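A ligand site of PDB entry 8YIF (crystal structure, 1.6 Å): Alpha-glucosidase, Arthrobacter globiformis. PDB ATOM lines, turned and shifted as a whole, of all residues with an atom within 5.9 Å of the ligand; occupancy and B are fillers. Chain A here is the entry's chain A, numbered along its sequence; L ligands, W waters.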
ATOM      1  N   ASN A  65     -29.322  -0.617 -11.638  1.00  0.00           N
ATOM      2  CA  ASN A  65     -28.129   0.015 -12.148  1.00  0.00           C
ATOM      3  C   ASN A  65     -28.427   1.479 -12.465  1.00  0.00           C
ATOM      4  O   ASN A  65     -29.597   1.869 -12.610  1.00  0.00           O
ATOM      5  CB  ASN A  65     -27.621  -0.766 -13.356  1.00  0.00           C
ATOM      6  CG  ASN A  65     -27.053  -2.109 -12.952  1.00  0.00           C
ATOM      7  OD1 ASN A  65     -27.689  -3.140 -13.119  1.00  0.00           O
ATOM      8  ND2 ASN A  65     -25.842  -2.091 -12.397  1.00  0.00           N
ATOM      9  N   ASP A  74     -20.094   5.242 -20.034  1.00  0.00           N
ATOM     10  CA  ASP A  74     -19.963   4.010 -19.261  1.00  0.00           C
ATOM     11  C   ASP A  74     -21.345   3.565 -18.816  1.00  0.00           C
ATOM     12  O   ASP A  74     -21.543   3.093 -17.704  1.00  0.00           O
ATOM     13  CB  ASP A  74     -19.019   4.203 -18.072  1.00  0.00           C
ATOM     14  CG  ASP A  74     -18.680   2.900 -17.370  1.00  0.00           C
ATOM     15  OD1 ASP A  74     -18.815   1.801 -17.967  1.00  0.00           O
ATOM     16  OD2 ASP A  74     -18.267   2.954 -16.196  1.00  0.00           O
ATOM     17  N   TYR A  77     -22.815   4.830 -15.458  1.00  0.00           N
ATOM     18  CA  TYR A  77     -21.850   5.089 -14.398  1.00  0.00           C
ATOM     19  C   TYR A  77     -21.044   6.358 -14.652  1.00  0.00           C
ATOM     20  O   TYR A  77     -20.152   6.681 -13.850  1.00  0.00           O
ATOM     21  CB  TYR A  77     -20.939   3.860 -14.204  1.00  0.00           C
ATOM     22  CG  TYR A  77     -21.663   2.739 -13.505  1.00  0.00           C
ATOM     23  CD1 TYR A  77     -21.778   2.722 -12.111  1.00  0.00           C
ATOM     24  CD2 TYR A  77     -22.285   1.714 -14.213  1.00  0.00           C
ATOM     25  CE1 TYR A  77     -22.480   1.722 -11.444  1.00  0.00           C
ATOM     26  CE2 TYR A  77     -22.981   0.694 -13.560  1.00  0.00           C
ATOM     27  CZ  TYR A  77     -23.067   0.708 -12.173  1.00  0.00           C
ATOM     28  OH  TYR A  77     -23.753  -0.274 -11.489  1.00  0.00           O
ATOM     29  N   ASP A  78     -21.370   7.088 -15.727  1.00  0.00           N
ATOM     30  CA  ASP A  78     -20.875   8.452 -15.970  1.00  0.00           C
ATOM     31  C   ASP A  78     -22.066   9.391 -15.858  1.00  0.00           C
ATOM     32  O   ASP A  78     -22.800   9.624 -16.828  1.00  0.00           O
ATOM     33  CB  ASP A  78     -20.183   8.586 -17.335  1.00  0.00           C
ATOM     34  CG  ASP A  78     -21.037   8.120 -18.505  1.00  0.00           C
ATOM     35  OD1 ASP A  78     -21.720   7.068 -18.426  1.00  0.00           O
ATOM     36  OD2 ASP A  78     -20.994   8.811 -19.544  1.00  0.00           O
ATOM     37  N   VAL A 114     -22.864   6.473  -7.307  1.00  0.00           N
ATOM     38  CA  VAL A 114     -21.642   6.548  -8.110  1.00  0.00           C
ATOM     39  C   VAL A 114     -20.948   7.850  -7.768  1.00  0.00           C
ATOM     40  O   VAL A 114     -21.068   8.840  -8.506  1.00  0.00           O
ATOM     41  CB  VAL A 114     -21.952   6.458  -9.614  1.00  0.00           C
ATOM     42  CG1 VAL A 114     -20.660   6.261 -10.392  1.00  0.00           C
ATOM     43  CG2 VAL A 114     -22.928   5.309  -9.888  1.00  0.00           C
ATOM     44  N   HIS A 117     -16.661   9.443  -9.092  1.00  0.00           N
ATOM     45  CA  HIS A 117     -16.416  10.189 -10.319  1.00  0.00           C
ATOM     46  C   HIS A 117     -17.773  10.604 -10.877  1.00  0.00           C
ATOM     47  O   HIS A 117     -18.809  10.006 -10.532  1.00  0.00           O
ATOM     48  CB  HIS A 117     -15.660   9.324 -11.350  1.00  0.00           C
ATOM     49  CG  HIS A 117     -16.246   7.962 -11.520  1.00  0.00           C
ATOM     50  ND1 HIS A 117     -15.796   6.876 -10.800  1.00  0.00           N
ATOM     51  CD2 HIS A 117     -17.287   7.518 -12.259  1.00  0.00           C
ATOM     52  CE1 HIS A 117     -16.514   5.804 -11.121  1.00  0.00           C
ATOM     53  NE2 HIS A 117     -17.420   6.176 -12.006  1.00  0.00           N
ATOM     54  N   VAL A 161      -8.582   1.726 -14.849  1.00  0.00           N
ATOM     55  CA  VAL A 161      -9.141   0.370 -14.743  1.00  0.00           C
ATOM     56  C   VAL A 161      -9.556  -0.155 -16.111  1.00  0.00           C
ATOM     57  O   VAL A 161      -9.525  -1.366 -16.357  1.00  0.00           O
ATOM     58  CB  VAL A 161     -10.328   0.374 -13.736  1.00  0.00           C
ATOM     59  CG1 VAL A 161     -11.004  -0.987 -13.698  1.00  0.00           C
ATOM     60  CG2 VAL A 161      -9.862   0.776 -12.338  1.00  0.00           C
ATOM     61  N   PHE A 162      -9.933   0.738 -17.024  1.00  0.00           N
ATOM     62  CA  PHE A 162     -10.396   0.342 -18.348  1.00  0.00           C
ATOM     63  C   PHE A 162      -9.264   0.269 -19.362  1.00  0.00           C
ATOM     64  O   PHE A 162      -9.527   0.133 -20.558  1.00  0.00           O
ATOM     65  CB  PHE A 162     -11.461   1.309 -18.854  1.00  0.00           C
ATOM     66  CG  PHE A 162     -12.752   1.276 -18.069  1.00  0.00           C
ATOM     67  CD1 PHE A 162     -13.134   0.155 -17.323  1.00  0.00           C
ATOM     68  CD2 PHE A 162     -13.615   2.357 -18.118  1.00  0.00           C
ATOM     69  CE1 PHE A 162     -14.347   0.154 -16.623  1.00  0.00           C
ATOM     70  CE2 PHE A 162     -14.816   2.355 -17.412  1.00  0.00           C
ATOM     71  CZ  PHE A 162     -15.179   1.245 -16.672  1.00  0.00           C
ATOM     72  N   PHE A 185     -11.450   5.484 -14.172  1.00  0.00           N
ATOM     73  CA  PHE A 185     -12.148   4.696 -15.179  1.00  0.00           C
ATOM     74  C   PHE A 185     -12.006   5.411 -16.533  1.00  0.00           C
ATOM     75  O   PHE A 185     -10.862   5.689 -16.931  1.00  0.00           O
ATOM     76  CB  PHE A 185     -13.567   4.440 -14.691  1.00  0.00           C
ATOM     77  CG  PHE A 185     -13.599   3.609 -13.453  1.00  0.00           C
ATOM     78  CD1 PHE A 185     -13.576   2.220 -13.527  1.00  0.00           C
ATOM     79  CD2 PHE A 185     -13.555   4.207 -12.191  1.00  0.00           C
ATOM     80  CE1 PHE A 185     -13.540   1.441 -12.371  1.00  0.00           C
ATOM     81  CE2 PHE A 185     -13.551   3.439 -11.035  1.00  0.00           C
ATOM     82  CZ  PHE A 185     -13.543   2.061 -11.125  1.00  0.00           C
ATOM     83  N   GLN A 189     -14.924  10.119 -17.219  1.00  0.00           N
ATOM     84  CA  GLN A 189     -15.324   9.948 -15.825  1.00  0.00           C
ATOM     85  C   GLN A 189     -14.265  10.543 -14.904  1.00  0.00           C
ATOM     86  O   GLN A 189     -13.570   9.823 -14.180  1.00  0.00           O
ATOM     87  CB  GLN A 189     -15.558   8.474 -15.494  1.00  0.00           C
ATOM     88  CG  GLN A 189     -16.784   7.841 -16.184  1.00  0.00           C
ATOM     89  CD  GLN A 189     -16.761   6.316 -16.129  1.00  0.00           C
ATOM     90  OE1 GLN A 189     -15.881   5.677 -16.714  1.00  0.00           O
ATOM     91  NE2 GLN A 189     -17.714   5.730 -15.431  1.00  0.00           N
ATOM     92  N   ARG A 219     -26.705   0.605  -3.333  1.00  0.00           N
ATOM     93  CA  ARG A 219     -25.483  -0.114  -3.675  1.00  0.00           C
ATOM     94  C   ARG A 219     -24.413   0.914  -4.018  1.00  0.00           C
ATOM     95  O   ARG A 219     -24.664   1.820  -4.833  1.00  0.00           O
ATOM     96  CB  ARG A 219     -25.765  -1.041  -4.856  1.00  0.00           C
ATOM     97  CG  ARG A 219     -24.553  -1.810  -5.387  1.00  0.00           C
ATOM     98  CD  ARG A 219     -23.890  -1.046  -6.529  1.00  0.00           C
ATOM     99  NE  ARG A 219     -22.893  -1.883  -7.204  1.00  0.00           N
ATOM    100  CZ  ARG A 219     -22.080  -1.433  -8.138  1.00  0.00           C
ATOM    101  NH1 ARG A 219     -22.058  -0.155  -8.474  1.00  0.00           N
ATOM    102  NH2 ARG A 219     -21.267  -2.289  -8.765  1.00  0.00           N
ATOM    103  N   ASP A 221     -21.104   2.101  -5.658  1.00  0.00           N
ATOM    104  CA  ASP A 221     -20.146   1.834  -6.720  1.00  0.00           C
ATOM    105  C   ASP A 221     -18.737   2.225  -6.271  1.00  0.00           C
ATOM    106  O   ASP A 221     -18.559   3.283  -5.670  1.00  0.00           O
ATOM    107  CB  ASP A 221     -20.554   2.644  -7.954  1.00  0.00           C
ATOM    108  CG  ASP A 221     -19.723   2.317  -9.179  1.00  0.00           C
ATOM    109  OD1 ASP A 221     -19.734   1.156  -9.587  1.00  0.00           O
ATOM    110  OD2 ASP A 221     -19.115   3.244  -9.745  1.00  0.00           O
ATOM    111  N   VAL A 222     -17.736   1.391  -6.611  1.00  0.00           N
ATOM    112  CA  VAL A 222     -16.343   1.614  -6.209  1.00  0.00           C
ATOM    113  C   VAL A 222     -16.234   2.030  -4.747  1.00  0.00           C
ATOM    114  O   VAL A 222     -15.722   3.115  -4.411  1.00  0.00           O
ATOM    115  CB  VAL A 222     -15.657   2.657  -7.121  1.00  0.00           C
ATOM    116  CG1 VAL A 222     -14.130   2.484  -7.078  1.00  0.00           C
ATOM    117  CG2 VAL A 222     -16.128   2.487  -8.567  1.00  0.00           C
ATOM    118  N   ALA A 223     -16.732   1.184  -3.843  1.00  0.00           N
ATOM    119  CA  ALA A 223     -16.747   1.596  -2.436  1.00  0.00           C
ATOM    120  C   ALA A 223     -15.332   1.721  -1.867  1.00  0.00           C
ATOM    121  O   ALA A 223     -15.142   2.429  -0.868  1.00  0.00           O
ATOM    122  CB  ALA A 223     -17.589   0.621  -1.617  1.00  0.00           C
ATOM    123  N   HIS A 224     -14.337   1.081  -2.488  1.00  0.00           N
ATOM    124  CA  HIS A 224     -12.945   1.255  -2.120  1.00  0.00           C
ATOM    125  C   HIS A 224     -12.324   2.486  -2.748  1.00  0.00           C
ATOM    126  O   HIS A 224     -11.112   2.706  -2.613  1.00  0.00           O
ATOM    127  CB  HIS A 224     -12.151   0.007  -2.510  1.00  0.00           C
ATOM    128  CG  HIS A 224     -12.267  -0.329  -3.965  1.00  0.00           C
ATOM    129  ND1 HIS A 224     -13.442  -0.779  -4.535  1.00  0.00           N
ATOM    130  CD2 HIS A 224     -11.376  -0.247  -4.976  1.00  0.00           C
ATOM    131  CE1 HIS A 224     -13.266  -0.969  -5.835  1.00  0.00           C
ATOM    132  NE2 HIS A 224     -12.014  -0.649  -6.129  1.00  0.00           N
ATOM    133  N   TRP A 250      -6.477   3.572  -3.954  1.00  0.00           N
ATOM    134  CA  TRP A 250      -7.691   2.978  -3.413  1.00  0.00           C
ATOM    135  C   TRP A 250      -7.579   2.821  -1.900  1.00  0.00           C
ATOM    136  O   TRP A 250      -6.500   2.912  -1.330  1.00  0.00           O
ATOM    137  CB  TRP A 250      -7.946   1.569  -3.988  1.00  0.00           C
ATOM    138  CG  TRP A 250      -7.792   1.458  -5.455  1.00  0.00           C
ATOM    139  CD1 TRP A 250      -6.778   0.840  -6.113  1.00  0.00           C
ATOM    140  CD2 TRP A 250      -8.693   1.946  -6.452  1.00  0.00           C
ATOM    141  NE1 TRP A 250      -6.969   0.921  -7.479  1.00  0.00           N
ATOM    142  CE2 TRP A 250      -8.137   1.596  -7.715  1.00  0.00           C
ATOM    143  CE3 TRP A 250      -9.887   2.658  -6.414  1.00  0.00           C
ATOM    144  CZ2 TRP A 250      -8.757   1.938  -8.916  1.00  0.00           C
ATOM    145  CZ3 TRP A 250     -10.510   2.991  -7.625  1.00  0.00           C
ATOM    146  CH2 TRP A 250      -9.933   2.619  -8.854  1.00  0.00           C
ATOM    147  N   GLU A 278     -19.851  -2.189  -3.239  1.00  0.00           N
ATOM    148  CA  GLU A 278     -19.067  -2.895  -4.249  1.00  0.00           C
ATOM    149  C   GLU A 278     -17.600  -2.659  -3.943  1.00  0.00           C
ATOM    150  O   GLU A 278     -17.042  -1.612  -4.277  1.00  0.00           O
ATOM    151  CB  GLU A 278     -19.417  -2.419  -5.656  1.00  0.00           C
ATOM    152  CG  GLU A 278     -18.734  -3.321  -6.718  1.00  0.00           C
ATOM    153  CD  GLU A 278     -18.123  -2.595  -7.886  1.00  0.00           C
ATOM    154  OE1 GLU A 278     -17.837  -1.393  -7.797  1.00  0.00           O
ATOM    155  OE2 GLU A 278     -17.879  -3.290  -8.910  1.00  0.00           O
ATOM    156  N   TRP A 280     -13.611  -3.983  -4.080  1.00  0.00           N
ATOM    157  CA  TRP A 280     -12.572  -4.867  -4.624  1.00  0.00           C
ATOM    158  C   TRP A 280     -11.241  -4.516  -3.963  1.00  0.00           C
ATOM    159  O   TRP A 280     -10.543  -3.606  -4.412  1.00  0.00           O
ATOM    160  CB  TRP A 280     -12.463  -4.725  -6.136  1.00  0.00           C
ATOM    161  CG  TRP A 280     -13.661  -5.144  -6.907  1.00  0.00           C
ATOM    162  CD1 TRP A 280     -14.751  -4.368  -7.195  1.00  0.00           C
ATOM    163  CD2 TRP A 280     -13.901  -6.422  -7.501  1.00  0.00           C
ATOM    164  NE1 TRP A 280     -15.658  -5.094  -7.941  1.00  0.00           N
ATOM    165  CE2 TRP A 280     -15.160  -6.346  -8.141  1.00  0.00           C
ATOM    166  CE3 TRP A 280     -13.168  -7.615  -7.563  1.00  0.00           C
ATOM    167  CZ2 TRP A 280     -15.705  -7.432  -8.835  1.00  0.00           C
ATOM    168  CZ3 TRP A 280     -13.713  -8.692  -8.257  1.00  0.00           C
ATOM    169  CH2 TRP A 280     -14.975  -8.597  -8.873  1.00  0.00           C
ATOM    170  N   HIS A 336     -23.327  -7.239 -13.983  1.00  0.00           N
ATOM    171  CA  HIS A 336     -23.184  -6.568 -15.266  1.00  0.00           C
ATOM    172  C   HIS A 336     -21.721  -6.346 -15.687  1.00  0.00           C
ATOM    173  O   HIS A 336     -21.490  -5.767 -16.761  1.00  0.00           O
ATOM    174  CB  HIS A 336     -23.929  -5.234 -15.213  1.00  0.00           C
ATOM    175  CG  HIS A 336     -23.377  -4.293 -14.203  1.00  0.00           C
ATOM    176  ND1 HIS A 336     -23.301  -4.601 -12.866  1.00  0.00           N
ATOM    177  CD2 HIS A 336     -22.789  -3.076 -14.348  1.00  0.00           C
ATOM    178  CE1 HIS A 336     -22.711  -3.613 -12.224  1.00  0.00           C
ATOM    179  NE2 HIS A 336     -22.391  -2.675 -13.096  1.00  0.00           N
ATOM    180  N   ASP A 337     -20.749  -6.785 -14.889  1.00  0.00           N
ATOM    181  CA  ASP A 337     -19.329  -6.560 -15.148  1.00  0.00           C
ATOM    182  C   ASP A 337     -18.558  -7.829 -15.511  1.00  0.00           C
ATOM    183  O   ASP A 337     -17.365  -7.738 -15.788  1.00  0.00           O
ATOM    184  CB  ASP A 337     -18.636  -5.942 -13.928  1.00  0.00           C
ATOM    185  CG  ASP A 337     -19.017  -4.484 -13.692  1.00  0.00           C
ATOM    186  OD1 ASP A 337     -19.426  -3.779 -14.636  1.00  0.00           O
ATOM    187  OD2 ASP A 337     -18.817  -4.035 -12.532  1.00  0.00           O
ATOM    188  N   ILE A 360     -10.751 -10.149 -11.163  1.00  0.00           N
ATOM    189  CA  ILE A 360     -11.934 -10.164 -12.022  1.00  0.00           C
ATOM    190  C   ILE A 360     -11.656 -10.834 -13.360  1.00  0.00           C
ATOM    191  O   ILE A 360     -12.594 -11.315 -14.009  1.00  0.00           O
ATOM    192  CB  ILE A 360     -12.479  -8.721 -12.228  1.00  0.00           C
ATOM    193  CG1 ILE A 360     -13.925  -8.758 -12.729  1.00  0.00           C
ATOM    194  CG2 ILE A 360     -11.615  -7.929 -13.201  1.00  0.00           C
ATOM    195  CD1 ILE A 360     -14.656  -7.438 -12.598  1.00  0.00           C
ATOM    196  N   ARG A 364     -13.824 -13.560 -16.735  1.00  0.00           N
ATOM    197  CA  ARG A 364     -13.949 -13.020 -18.096  1.00  0.00           C
ATOM    198  C   ARG A 364     -13.171 -13.867 -19.091  1.00  0.00           C
ATOM    199  O   ARG A 364     -12.698 -13.336 -20.099  1.00  0.00           O
ATOM    200  CB  ARG A 364     -13.461 -11.574 -18.164  1.00  0.00           C
ATOM    201  CG  ARG A 364     -14.323 -10.595 -17.366  1.00  0.00           C
ATOM    202  CD  ARG A 364     -13.602  -9.262 -17.263  1.00  0.00           C
ATOM    203  NE  ARG A 364     -14.501  -8.205 -16.807  1.00  0.00           N
ATOM    204  CZ  ARG A 364     -14.088  -7.022 -16.391  1.00  0.00           C
ATOM    205  NH1 ARG A 364     -12.804  -6.709 -16.358  1.00  0.00           N
ATOM    206  NH2 ARG A 364     -14.991  -6.134 -15.975  1.00  0.00           N
ATOM    207  N   ILE A 417     -14.178  -0.409 -22.343  1.00  0.00           N
ATOM    208  CA  ILE A 417     -13.094  -1.394 -22.296  1.00  0.00           C
ATOM    209  C   ILE A 417     -12.713  -1.832 -23.708  1.00  0.00           C
ATOM    210  O   ILE A 417     -11.528  -2.010 -24.039  1.00  0.00           O
ATOM    211  CB  ILE A 417     -13.479  -2.600 -21.428  1.00  0.00           C
ATOM    212  CG1 ILE A 417     -13.498  -2.213 -19.937  1.00  0.00           C
ATOM    213  CG2 ILE A 417     -12.504  -3.770 -21.651  1.00  0.00           C
ATOM    214  CD1 ILE A 417     -14.117  -3.284 -19.079  1.00  0.00           C
ATOM    215  N   ARG A 428     -17.832  -5.882 -21.587  1.00  0.00           N
ATOM    216  CA  ARG A 428     -18.952  -6.398 -20.821  1.00  0.00           C
ATOM    217  C   ARG A 428     -20.275  -6.394 -21.591  1.00  0.00           C
ATOM    218  O   ARG A 428     -21.314  -6.733 -20.999  1.00  0.00           O
ATOM    219  CB  ARG A 428     -19.122  -5.556 -19.540  1.00  0.00           C
ATOM    220  CG  ARG A 428     -17.902  -5.603 -18.664  1.00  0.00           C
ATOM    221  CD  ARG A 428     -17.841  -4.421 -17.681  1.00  0.00           C
ATOM    222  NE  ARG A 428     -17.589  -3.142 -18.345  1.00  0.00           N
ATOM    223  CZ  ARG A 428     -17.592  -1.971 -17.720  1.00  0.00           C
ATOM    224  NH1 ARG A 428     -17.828  -1.891 -16.408  1.00  0.00           N
ATOM    225  NH2 ARG A 428     -17.363  -0.860 -18.418  1.00  0.00           N
ATOM    226  N   ARG A 432     -25.090  -7.766 -21.284  1.00  0.00           N
ATOM    227  CA  ARG A 432     -26.010  -6.638 -21.249  1.00  0.00           C
ATOM    228  C   ARG A 432     -26.980  -6.662 -22.420  1.00  0.00           C
ATOM    229  O   ARG A 432     -27.589  -5.632 -22.755  1.00  0.00           O
ATOM    230  CB  ARG A 432     -25.206  -5.324 -21.216  1.00  0.00           C
ATOM    231  CG  ARG A 432     -24.356  -5.212 -19.959  1.00  0.00           C
ATOM    232  CD  ARG A 432     -23.405  -4.045 -20.055  1.00  0.00           C
ATOM    233  NE  ARG A 432     -22.513  -3.939 -18.896  1.00  0.00           N
ATOM    234  CZ  ARG A 432     -21.722  -2.894 -18.674  1.00  0.00           C
ATOM    235  NH1 ARG A 432     -21.626  -1.911 -19.556  1.00  0.00           N
ATOM    236  NH2 ARG A 432     -20.999  -2.854 -17.548  1.00  0.00           N
HETATM  237  C1  LIG L   1     -12.455  -5.310 -10.540  1.00  0.00           C
HETATM  238  O1  LIG L   1     -13.387  -4.231 -10.315  1.00  0.00           O
HETATM  239  C2  LIG L   1     -13.095  -3.013 -10.952  1.00  0.00           C
HETATM  240  O2  LIG L   1     -12.890  -2.063  -8.776  1.00  0.00           O
HETATM  241  C3  LIG L   1     -13.529  -1.889 -10.033  1.00  0.00           C
HETATM  242  C4  LIG L   1     -18.541   0.631 -13.646  1.00  0.00           C
HETATM  243  C5  LIG L   1     -15.045  -1.906  -9.879  1.00  0.00           C
HETATM  244  O3  LIG L   1     -15.446  -0.796  -9.087  1.00  0.00           O
HETATM  245  C6  LIG L   1     -15.721  -1.866 -11.247  1.00  0.00           C
HETATM  246  N1  LIG L   1     -17.185  -1.992 -11.158  1.00  0.00           N
HETATM  247  C7  LIG L   1     -15.187  -3.005 -12.115  1.00  0.00           C
HETATM  248  O4  LIG L   1     -13.752  -2.949 -12.199  1.00  0.00           O
HETATM  249  C8  LIG L   1     -15.681  -2.945 -13.541  1.00  0.00           C
HETATM  250  C9  LIG L   1     -17.986  -0.738 -11.081  1.00  0.00           C
HETATM  251  C10 LIG L   1     -19.331  -0.855 -11.820  1.00  0.00           C
HETATM  252  O5  LIG L   1     -20.046  -2.021 -11.452  1.00  0.00           O
HETATM  253  C11 LIG L   1     -18.971  -0.799 -13.302  1.00  0.00           C
HETATM  254  O6  LIG L   1     -20.061  -1.188 -14.128  1.00  0.00           O
HETATM  255  O7  LIG L   1     -18.049   0.727 -14.980  1.00  0.00           O
HETATM  256  C12 LIG L   1     -17.566   1.193 -12.626  1.00  0.00           C
HETATM  257  C13 LIG L   1     -17.240   0.492 -11.549  1.00  0.00           C
HETATM  258  C14 LIG L   1     -17.226   2.646 -12.792  1.00  0.00           C
HETATM  259  O8  LIG L   1     -18.275   3.497 -12.373  1.00  0.00           O
HETATM  260  O   HOH W   1      -9.870  -7.583  -9.937  1.00  0.00           O
HETATM  261  O   HOH W   2     -12.820  -4.189 -15.045  1.00  0.00           O
HETATM  262  O   HOH W   3     -20.554  -0.079 -16.728  1.00  0.00           O
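OD2 of Asp 74 sits at hydrogen-bond distance from O7 of the ligand, at 2.5 Å. A nitrogen (N1) of the ligand lies within salt-bridge range of the side-chain carboxylate of Asp 337 (3.0 Å). OE2 of Glu 278 is in salt-bridge range of N1 of the ligand, at 2.7 Å. The side-chain carboxylate (OD2) of Asp 221 lies within hydrogen-bond range of an oxygen (O8) of the ligand (2.8 Å). An oxygen (O8) of the ligand lies within hydrogen-bond range of a ring nitrogen (NE2) of His 117 (2.8 Å). NE2 of His 336 sits at hydrogen-bond distance from O5 of the ligand (2.9 Å). O5 of the ligand is in hydrogen-bond range of NH2 of Arg 219 (3.0 Å). O7 of the ligand sits at hydrogen-bond distance from NH1 of Arg 428 (3.0 Å). NE2 of His 224 is in hydrogen-bond range of O2 of the ligand, 3.1 Å away. The indole nitrogen of Trp 280 sits at hydrogen-bond distance from an oxygen (O1) of the ligand, 3.4 Å away.
OD1 of Asp 74 is in salt-bridge range of NH2 of Arg 428. The side-chain carboxylate (OD2) of Asp 74 lies within hydrogen-bond range of the side-chain amide nitrogen (NE2) of Gln 189, at 2.9 Å. The side-chain carboxylate of Asp 337 lies within salt-bridge range of the guanidinium group of Arg 428. OD1 of Asp 221 is in salt-bridge range of NH1 of Arg 219. NE of Arg 432 lies within hydrogen-bond range of O of His 336. The guanidinium group of Arg 219 is in hydrogen-bond range of the side-chain hydroxyl of Tyr 77 (3.5 Å). The backbone NH (N) of Trp 280 is in hydrogen-bond range of a ring nitrogen (ND1) of His 224, 3.2 Å away. The side-chain amide nitrogen (NE2) of Gln 189 sits at hydrogen-bond distance from the backbone carbonyl oxygen (O) of Tyr 77.
Merely in contact with the ligand: Tyr 77 (3.3 Å), Val 161 (3.7 Å), Phe 162 (3.4 Å), Phe 185 (3.7 Å), Gln 189 (3.8 Å), Val 222 (3.4 Å), Ile 360 (3.7 Å) and Arg 432 (3.9 Å). Hydrophobic or aromatic side chains within 4 Å of the ligand: Tyr 77, His 117, Val 161, Phe 162, Phe 185, Val 222, His 224, Trp 280, His 336 and Ile 360. Of the 25 residues printed, 18 come within 4 Å of the ligand.
Water W3 lies within hydrogen-bond range of OD1 of Asp 74 (2.8 Å), O6 of the ligand (2.9 Å), NH2 of Arg 432 (2.9 Å) and NH1 of Arg 428 (3.3 Å). Water W2 bridges NH1 of Arg 364 (2.8 Å) and O4 of the ligand (3.2 Å).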
